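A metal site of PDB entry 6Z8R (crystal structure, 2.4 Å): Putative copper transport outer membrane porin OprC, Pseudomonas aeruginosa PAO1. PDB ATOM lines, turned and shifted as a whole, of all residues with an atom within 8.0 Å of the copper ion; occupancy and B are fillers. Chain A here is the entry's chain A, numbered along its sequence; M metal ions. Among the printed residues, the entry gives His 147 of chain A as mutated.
The backbone NH (N) of His 323 lies within hydrogen-bond range of the backbone carbonyl oxygen (O) of Val 347, 2.8 Å away. The side-chain carboxylate (OD1) of Asp 148 lies within hydrogen-bond range of the backbone NH (N) of Cys 143 (2.9 Å). The backbone carbonyl oxygen (O) of Met 325 lies within hydrogen-bond range of the backbone NH (N) of Ser 345, at 2.9 Å. O of Met 286 lies within hydrogen-bond range of NE2 of His 147, 3.2 Å away. SG of Cys 143 lies close to N of Asn 145, at 3.3 Å. SG of Cys 143 sits close to N of His 147 (3.5 Å). OH of Tyr 281 sits at hydrogen-bond distance from O of His 147 (2.9 Å). A ring nitrogen (ND1) of His 323 lies within hydrogen-bond range of the backbone carbonyl oxygen of Gln 290, at 3.1 Å.
His 147 touches the copper ion. Within 4 Å of the copper ion: Cys 143, His 147, His 323 and Met 325. The nearest printed residue that does not touch the copper ion is Pro 144 (5.1 Å).
The copper ion is bound by NE2 of His 323 (2.2 Å), SG of Cys 143 (2.3 Å) and SD of Met 325 (2.4 Å). The copper ion has three donor atoms within binding distance.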
ATOM      1  N   ALA A 142     -15.690  28.511  19.653  1.00  0.00           N
ATOM      2  CA  ALA A 142     -14.444  29.221  19.488  1.00  0.00           C
ATOM      3  C   ALA A 142     -14.312  29.954  18.161  1.00  0.00           C
ATOM      4  O   ALA A 142     -13.441  30.831  18.051  1.00  0.00           O
ATOM      5  CB  ALA A 142     -13.262  28.251  19.629  1.00  0.00           C
ATOM      6  N   CYS A 143     -15.126  29.625  17.175  1.00  0.00           N
ATOM      7  CA  CYS A 143     -14.957  30.220  15.854  1.00  0.00           C
ATOM      8  C   CYS A 143     -15.325  31.696  15.883  1.00  0.00           C
ATOM      9  O   CYS A 143     -16.411  32.039  16.361  1.00  0.00           O
ATOM     10  CB  CYS A 143     -15.821  29.498  14.833  1.00  0.00           C
ATOM     11  SG  CYS A 143     -15.640  30.198  13.201  1.00  0.00           S
ATOM     12  N   PRO A 144     -14.479  32.597  15.375  1.00  0.00           N
ATOM     13  CA  PRO A 144     -14.873  34.024  15.322  1.00  0.00           C
ATOM     14  C   PRO A 144     -16.017  34.316  14.368  1.00  0.00           C
ATOM     15  O   PRO A 144     -16.536  35.427  14.406  1.00  0.00           O
ATOM     16  CB  PRO A 144     -13.584  34.733  14.859  1.00  0.00           C
ATOM     17  CG  PRO A 144     -12.559  33.748  14.786  1.00  0.00           C
ATOM     18  CD  PRO A 144     -13.144  32.381  14.813  1.00  0.00           C
ATOM     19  N   ASN A 145     -16.404  33.375  13.508  1.00  0.00           N
ATOM     20  CA  ASN A 145     -17.562  33.527  12.627  1.00  0.00           C
ATOM     21  C   ASN A 145     -18.763  32.695  13.076  1.00  0.00           C
ATOM     22  O   ASN A 145     -19.716  32.517  12.307  1.00  0.00           O
ATOM     23  CB  ASN A 145     -17.183  33.128  11.195  1.00  0.00           C
ATOM     24  CG  ASN A 145     -16.066  33.955  10.669  1.00  0.00           C
ATOM     25  OD1 ASN A 145     -14.927  33.493  10.547  1.00  0.00           O
ATOM     26  ND2 ASN A 145     -16.362  35.199  10.351  1.00  0.00           N
ATOM     27  N   ARG A 146     -18.716  32.155  14.299  1.00  0.00           N
ATOM     28  CA  ARG A 146     -19.722  31.255  14.843  1.00  0.00           C
ATOM     29  C   ARG A 146     -20.088  30.102  13.881  1.00  0.00           C
ATOM     30  O   ARG A 146     -21.262  29.744  13.733  1.00  0.00           O
ATOM     31  CB  ARG A 146     -20.953  32.033  15.271  1.00  0.00           C
ATOM     32  CG  ARG A 146     -20.671  32.969  16.415  1.00  0.00           C
ATOM     33  CD  ARG A 146     -21.926  33.739  16.799  1.00  0.00           C
ATOM     34  NE  ARG A 146     -23.065  32.877  17.196  1.00  0.00           N
ATOM     35  CZ  ARG A 146     -23.389  32.610  18.460  1.00  0.00           C
ATOM     36  NH1 ARG A 146     -22.674  33.111  19.478  1.00  0.00           N
ATOM     37  NH2 ARG A 146     -24.447  31.852  18.717  1.00  0.00           N
ATOM     38  N   HIS A 147     -19.062  29.512  13.246  1.00  0.00           N
ATOM     39  CA  HIS A 147     -19.187  28.163  12.690  1.00  0.00           C
ATOM     40  C   HIS A 147     -19.738  27.170  13.711  1.00  0.00           C
ATOM     41  O   HIS A 147     -20.322  26.148  13.340  1.00  0.00           O
ATOM     42  CB  HIS A 147     -17.832  27.616  12.255  1.00  0.00           C
ATOM     43  CG  HIS A 147     -17.432  27.921  10.851  1.00  0.00           C
ATOM     44  ND1 HIS A 147     -17.685  29.137  10.244  1.00  0.00           N
ATOM     45  CD2 HIS A 147     -16.714  27.203   9.962  1.00  0.00           C
ATOM     46  CE1 HIS A 147     -17.176  29.125   9.024  1.00  0.00           C
ATOM     47  NE2 HIS A 147     -16.586  27.963   8.829  1.00  0.00           N
ATOM     48  N   ASP A 148     -19.484  27.412  14.987  1.00  0.00           N
ATOM     49  CA  ASP A 148     -19.681  26.420  16.032  1.00  0.00           C
ATOM     50  C   ASP A 148     -20.423  27.043  17.198  1.00  0.00           C
ATOM     51  O   ASP A 148     -19.980  27.010  18.354  1.00  0.00           O
ATOM     52  CB  ASP A 148     -18.331  25.816  16.481  1.00  0.00           C
ATOM     53  CG  ASP A 148     -17.407  26.837  17.165  1.00  0.00           C
ATOM     54  OD1 ASP A 148     -17.589  28.055  16.938  1.00  0.00           O
ATOM     55  OD2 ASP A 148     -16.532  26.435  17.961  1.00  0.00           O
ATOM     56  N   TYR A 281     -20.402  23.699   4.529  1.00  0.00           N
ATOM     57  CA  TYR A 281     -21.230  24.894   4.704  1.00  0.00           C
ATOM     58  C   TYR A 281     -21.473  25.583   3.359  1.00  0.00           C
ATOM     59  O   TYR A 281     -20.619  26.334   2.870  1.00  0.00           O
ATOM     60  CB  TYR A 281     -20.561  25.850   5.679  1.00  0.00           C
ATOM     61  CG  TYR A 281     -20.624  25.417   7.124  1.00  0.00           C
ATOM     62  CD1 TYR A 281     -21.762  24.784   7.626  1.00  0.00           C
ATOM     63  CD2 TYR A 281     -19.541  25.655   7.994  1.00  0.00           C
ATOM     64  CE1 TYR A 281     -21.840  24.404   8.959  1.00  0.00           C
ATOM     65  CE2 TYR A 281     -19.608  25.270   9.333  1.00  0.00           C
ATOM     66  CZ  TYR A 281     -20.752  24.649   9.809  1.00  0.00           C
ATOM     67  OH  TYR A 281     -20.831  24.272  11.129  1.00  0.00           O
ATOM     68  N   ARG A 284     -20.719  29.508   3.709  1.00  0.00           N
ATOM     69  CA  ARG A 284     -19.479  30.113   4.195  1.00  0.00           C
ATOM     70  C   ARG A 284     -18.374  29.952   3.162  1.00  0.00           C
ATOM     71  O   ARG A 284     -18.482  29.156   2.228  1.00  0.00           O
ATOM     72  CB  ARG A 284     -19.001  29.501   5.511  1.00  0.00           C
ATOM     73  CG  ARG A 284     -20.039  29.307   6.548  1.00  0.00           C
ATOM     74  CD  ARG A 284     -20.446  30.600   7.082  1.00  0.00           C
ATOM     75  NE  ARG A 284     -21.200  30.476   8.333  1.00  0.00           N
ATOM     76  CZ  ARG A 284     -20.864  31.092   9.453  1.00  0.00           C
ATOM     77  NH1 ARG A 284     -19.774  31.857   9.486  1.00  0.00           N
ATOM     78  NH2 ARG A 284     -21.588  30.939  10.545  1.00  0.00           N
ATOM     79  N   MET A 286     -15.513  28.805   4.189  1.00  0.00           N
ATOM     80  CA  MET A 286     -14.725  27.734   4.771  1.00  0.00           C
ATOM     81  C   MET A 286     -15.653  26.689   5.368  1.00  0.00           C
ATOM     82  O   MET A 286     -16.775  26.995   5.782  1.00  0.00           O
ATOM     83  CB  MET A 286     -13.771  28.293   5.856  1.00  0.00           C
ATOM     84  CG  MET A 286     -12.413  28.742   5.323  1.00  0.00           C
ATOM     85  SD  MET A 286     -11.283  29.273   6.650  1.00  0.00           S
ATOM     86  CE  MET A 286      -9.853  29.737   5.683  1.00  0.00           C
ATOM     87  N   ASP A 287     -15.192  25.447   5.435  1.00  0.00           N
ATOM     88  CA  ASP A 287     -15.949  24.417   6.130  1.00  0.00           C
ATOM     89  C   ASP A 287     -15.346  24.137   7.496  1.00  0.00           C
ATOM     90  O   ASP A 287     -14.162  24.403   7.747  1.00  0.00           O
ATOM     91  CB  ASP A 287     -16.008  23.126   5.317  1.00  0.00           C
ATOM     92  CG  ASP A 287     -16.383  23.366   3.863  1.00  0.00           C
ATOM     93  OD1 ASP A 287     -17.579  23.624   3.597  1.00  0.00           O
ATOM     94  OD2 ASP A 287     -15.469  23.302   3.001  1.00  0.00           O
ATOM     95  N   GLY A 288     -16.166  23.574   8.370  1.00  0.00           N
ATOM     96  CA  GLY A 288     -15.731  23.087   9.663  1.00  0.00           C
ATOM     97  C   GLY A 288     -15.267  21.655   9.582  1.00  0.00           C
ATOM     98  O   GLY A 288     -16.080  20.718   9.482  1.00  0.00           O
ATOM     99  N   SER A 289     -13.952  21.450   9.615  1.00  0.00           N
ATOM    100  CA  SER A 289     -13.431  20.093   9.555  1.00  0.00           C
ATOM    101  C   SER A 289     -13.217  19.478  10.923  1.00  0.00           C
ATOM    102  O   SER A 289     -12.832  18.304  11.000  1.00  0.00           O
ATOM    103  CB  SER A 289     -12.116  20.061   8.787  1.00  0.00           C
ATOM    104  OG  SER A 289     -11.207  21.002   9.339  1.00  0.00           O
ATOM    105  N   GLN A 290     -13.420  20.222  12.016  1.00  0.00           N
ATOM    106  CA  GLN A 290     -13.254  19.655  13.353  1.00  0.00           C
ATOM    107  C   GLN A 290     -14.056  20.488  14.348  1.00  0.00           C
ATOM    108  O   GLN A 290     -13.959  21.713  14.373  1.00  0.00           O
ATOM    109  CB  GLN A 290     -11.755  19.588  13.748  1.00  0.00           C
ATOM    110  CG  GLN A 290     -11.546  19.174  15.208  1.00  0.00           C
ATOM    111  CD  GLN A 290     -10.088  19.046  15.578  1.00  0.00           C
ATOM    112  OE1 GLN A 290      -9.394  18.121  15.124  1.00  0.00           O
ATOM    113  NE2 GLN A 290      -9.602  19.962  16.422  1.00  0.00           N
ATOM    114  N   PHE A 291     -14.853  19.800  15.180  1.00  0.00           N
ATOM    115  CA  PHE A 291     -15.580  20.424  16.281  1.00  0.00           C
ATOM    116  C   PHE A 291     -15.309  19.632  17.560  1.00  0.00           C
ATOM    117  O   PHE A 291     -16.203  18.978  18.100  1.00  0.00           O
ATOM    118  CB  PHE A 291     -17.092  20.479  16.007  1.00  0.00           C
ATOM    119  CG  PHE A 291     -17.475  21.327  14.837  1.00  0.00           C
ATOM    120  CD1 PHE A 291     -17.540  20.780  13.571  1.00  0.00           C
ATOM    121  CD2 PHE A 291     -17.790  22.645  15.012  1.00  0.00           C
ATOM    122  CE1 PHE A 291     -17.913  21.563  12.496  1.00  0.00           C
ATOM    123  CE2 PHE A 291     -18.157  23.431  13.945  1.00  0.00           C
ATOM    124  CZ  PHE A 291     -18.222  22.894  12.688  1.00  0.00           C
ATOM    125  N   HIS A 323     -11.757  23.919  17.402  1.00  0.00           N
ATOM    126  CA  HIS A 323     -12.424  23.969  16.114  1.00  0.00           C
ATOM    127  C   HIS A 323     -11.412  24.295  15.026  1.00  0.00           C
ATOM    128  O   HIS A 323     -10.567  25.175  15.199  1.00  0.00           O
ATOM    129  CB  HIS A 323     -13.515  25.026  16.161  1.00  0.00           C
ATOM    130  CG  HIS A 323     -14.032  25.451  14.823  1.00  0.00           C
ATOM    131  ND1 HIS A 323     -14.834  24.641  14.048  1.00  0.00           N
ATOM    132  CD2 HIS A 323     -13.882  26.614  14.140  1.00  0.00           C
ATOM    133  CE1 HIS A 323     -15.161  25.288  12.943  1.00  0.00           C
ATOM    134  NE2 HIS A 323     -14.590  26.481  12.974  1.00  0.00           N
ATOM    135  N   ILE A 324     -11.511  23.577  13.898  1.00  0.00           N
ATOM    136  CA  ILE A 324     -10.710  23.847  12.705  1.00  0.00           C
ATOM    137  C   ILE A 324     -11.642  24.121  11.523  1.00  0.00           C
ATOM    138  O   ILE A 324     -12.561  23.334  11.256  1.00  0.00           O
ATOM    139  CB  ILE A 324      -9.744  22.692  12.367  1.00  0.00           C
ATOM    140  CG1 ILE A 324      -8.734  22.476  13.493  1.00  0.00           C
ATOM    141  CG2 ILE A 324      -9.028  22.963  11.068  1.00  0.00           C
ATOM    142  CD1 ILE A 324      -8.074  21.107  13.433  1.00  0.00           C
ATOM    143  N   MET A 325     -11.395  25.211  10.814  1.00  0.00           N
ATOM    144  CA  MET A 325     -12.058  25.462   9.546  1.00  0.00           C
ATOM    145  C   MET A 325     -10.979  25.565   8.481  1.00  0.00           C
ATOM    146  O   MET A 325      -9.812  25.876   8.757  1.00  0.00           O
ATOM    147  CB  MET A 325     -12.846  26.763   9.546  1.00  0.00           C
ATOM    148  CG  MET A 325     -12.018  27.872   9.984  1.00  0.00           C
ATOM    149  SD  MET A 325     -13.030  29.273  10.591  1.00  0.00           S
ATOM    150  CE  MET A 325     -13.951  29.655   9.084  1.00  0.00           C
ATOM    151  N   ASP A 326     -11.364  25.295   7.240  1.00  0.00           N
ATOM    152  CA  ASP A 326     -10.414  25.376   6.139  1.00  0.00           C
ATOM    153  C   ASP A 326     -11.173  25.290   4.826  1.00  0.00           C
ATOM    154  O   ASP A 326     -12.372  25.010   4.804  1.00  0.00           O
ATOM    155  CB  ASP A 326      -9.336  24.304   6.227  1.00  0.00           C
ATOM    156  CG  ASP A 326      -9.905  22.887   6.193  1.00  0.00           C
ATOM    157  OD1 ASP A 326     -10.598  22.519   5.216  1.00  0.00           O
ATOM    158  OD2 ASP A 326      -9.634  22.120   7.144  1.00  0.00           O
ATOM    159  N   SER A 345      -7.615  27.487   9.720  1.00  0.00           N
ATOM    160  CA  SER A 345      -7.613  28.334  10.906  1.00  0.00           C
ATOM    161  C   SER A 345      -8.102  27.500  12.088  1.00  0.00           C
ATOM    162  O   SER A 345      -9.207  26.954  12.043  1.00  0.00           O
ATOM    163  CB  SER A 345      -8.495  29.558  10.677  1.00  0.00           C
ATOM    164  OG  SER A 345      -8.722  30.217  11.898  1.00  0.00           O
ATOM    165  N   GLN A 346      -7.269  27.388  13.133  1.00  0.00           N
ATOM    166  CA  GLN A 346      -7.602  26.638  14.334  1.00  0.00           C
ATOM    167  C   GLN A 346      -7.833  27.579  15.526  1.00  0.00           C
ATOM    168  O   GLN A 346      -7.093  28.557  15.709  1.00  0.00           O
ATOM    169  CB  GLN A 346      -6.499  25.637  14.681  1.00  0.00           C
ATOM    170  CG  GLN A 346      -6.915  24.642  15.754  1.00  0.00           C
ATOM    171  CD  GLN A 346      -5.907  23.580  16.012  1.00  0.00           C
ATOM    172  OE1 GLN A 346      -4.792  23.610  15.487  1.00  0.00           O
ATOM    173  NE2 GLN A 346      -6.273  22.606  16.828  1.00  0.00           N
ATOM    174  N   VAL A 347      -8.861  27.287  16.311  1.00  0.00           N
ATOM    175  CA  VAL A 347      -9.244  28.147  17.427  1.00  0.00           C
ATOM    176  C   VAL A 347      -9.763  27.268  18.543  1.00  0.00           C
ATOM    177  O   VAL A 347     -10.291  26.170  18.299  1.00  0.00           O
ATOM    178  CB  VAL A 347     -10.326  29.168  17.005  1.00  0.00           C
ATOM    179  CG1 VAL A 347      -9.737  30.266  16.141  1.00  0.00           C
ATOM    180  CG2 VAL A 347     -11.485  28.457  16.307  1.00  0.00           C
HETATM  181 CU    CU M   1     -14.758  28.409  12.013  1.00  0.00          CU
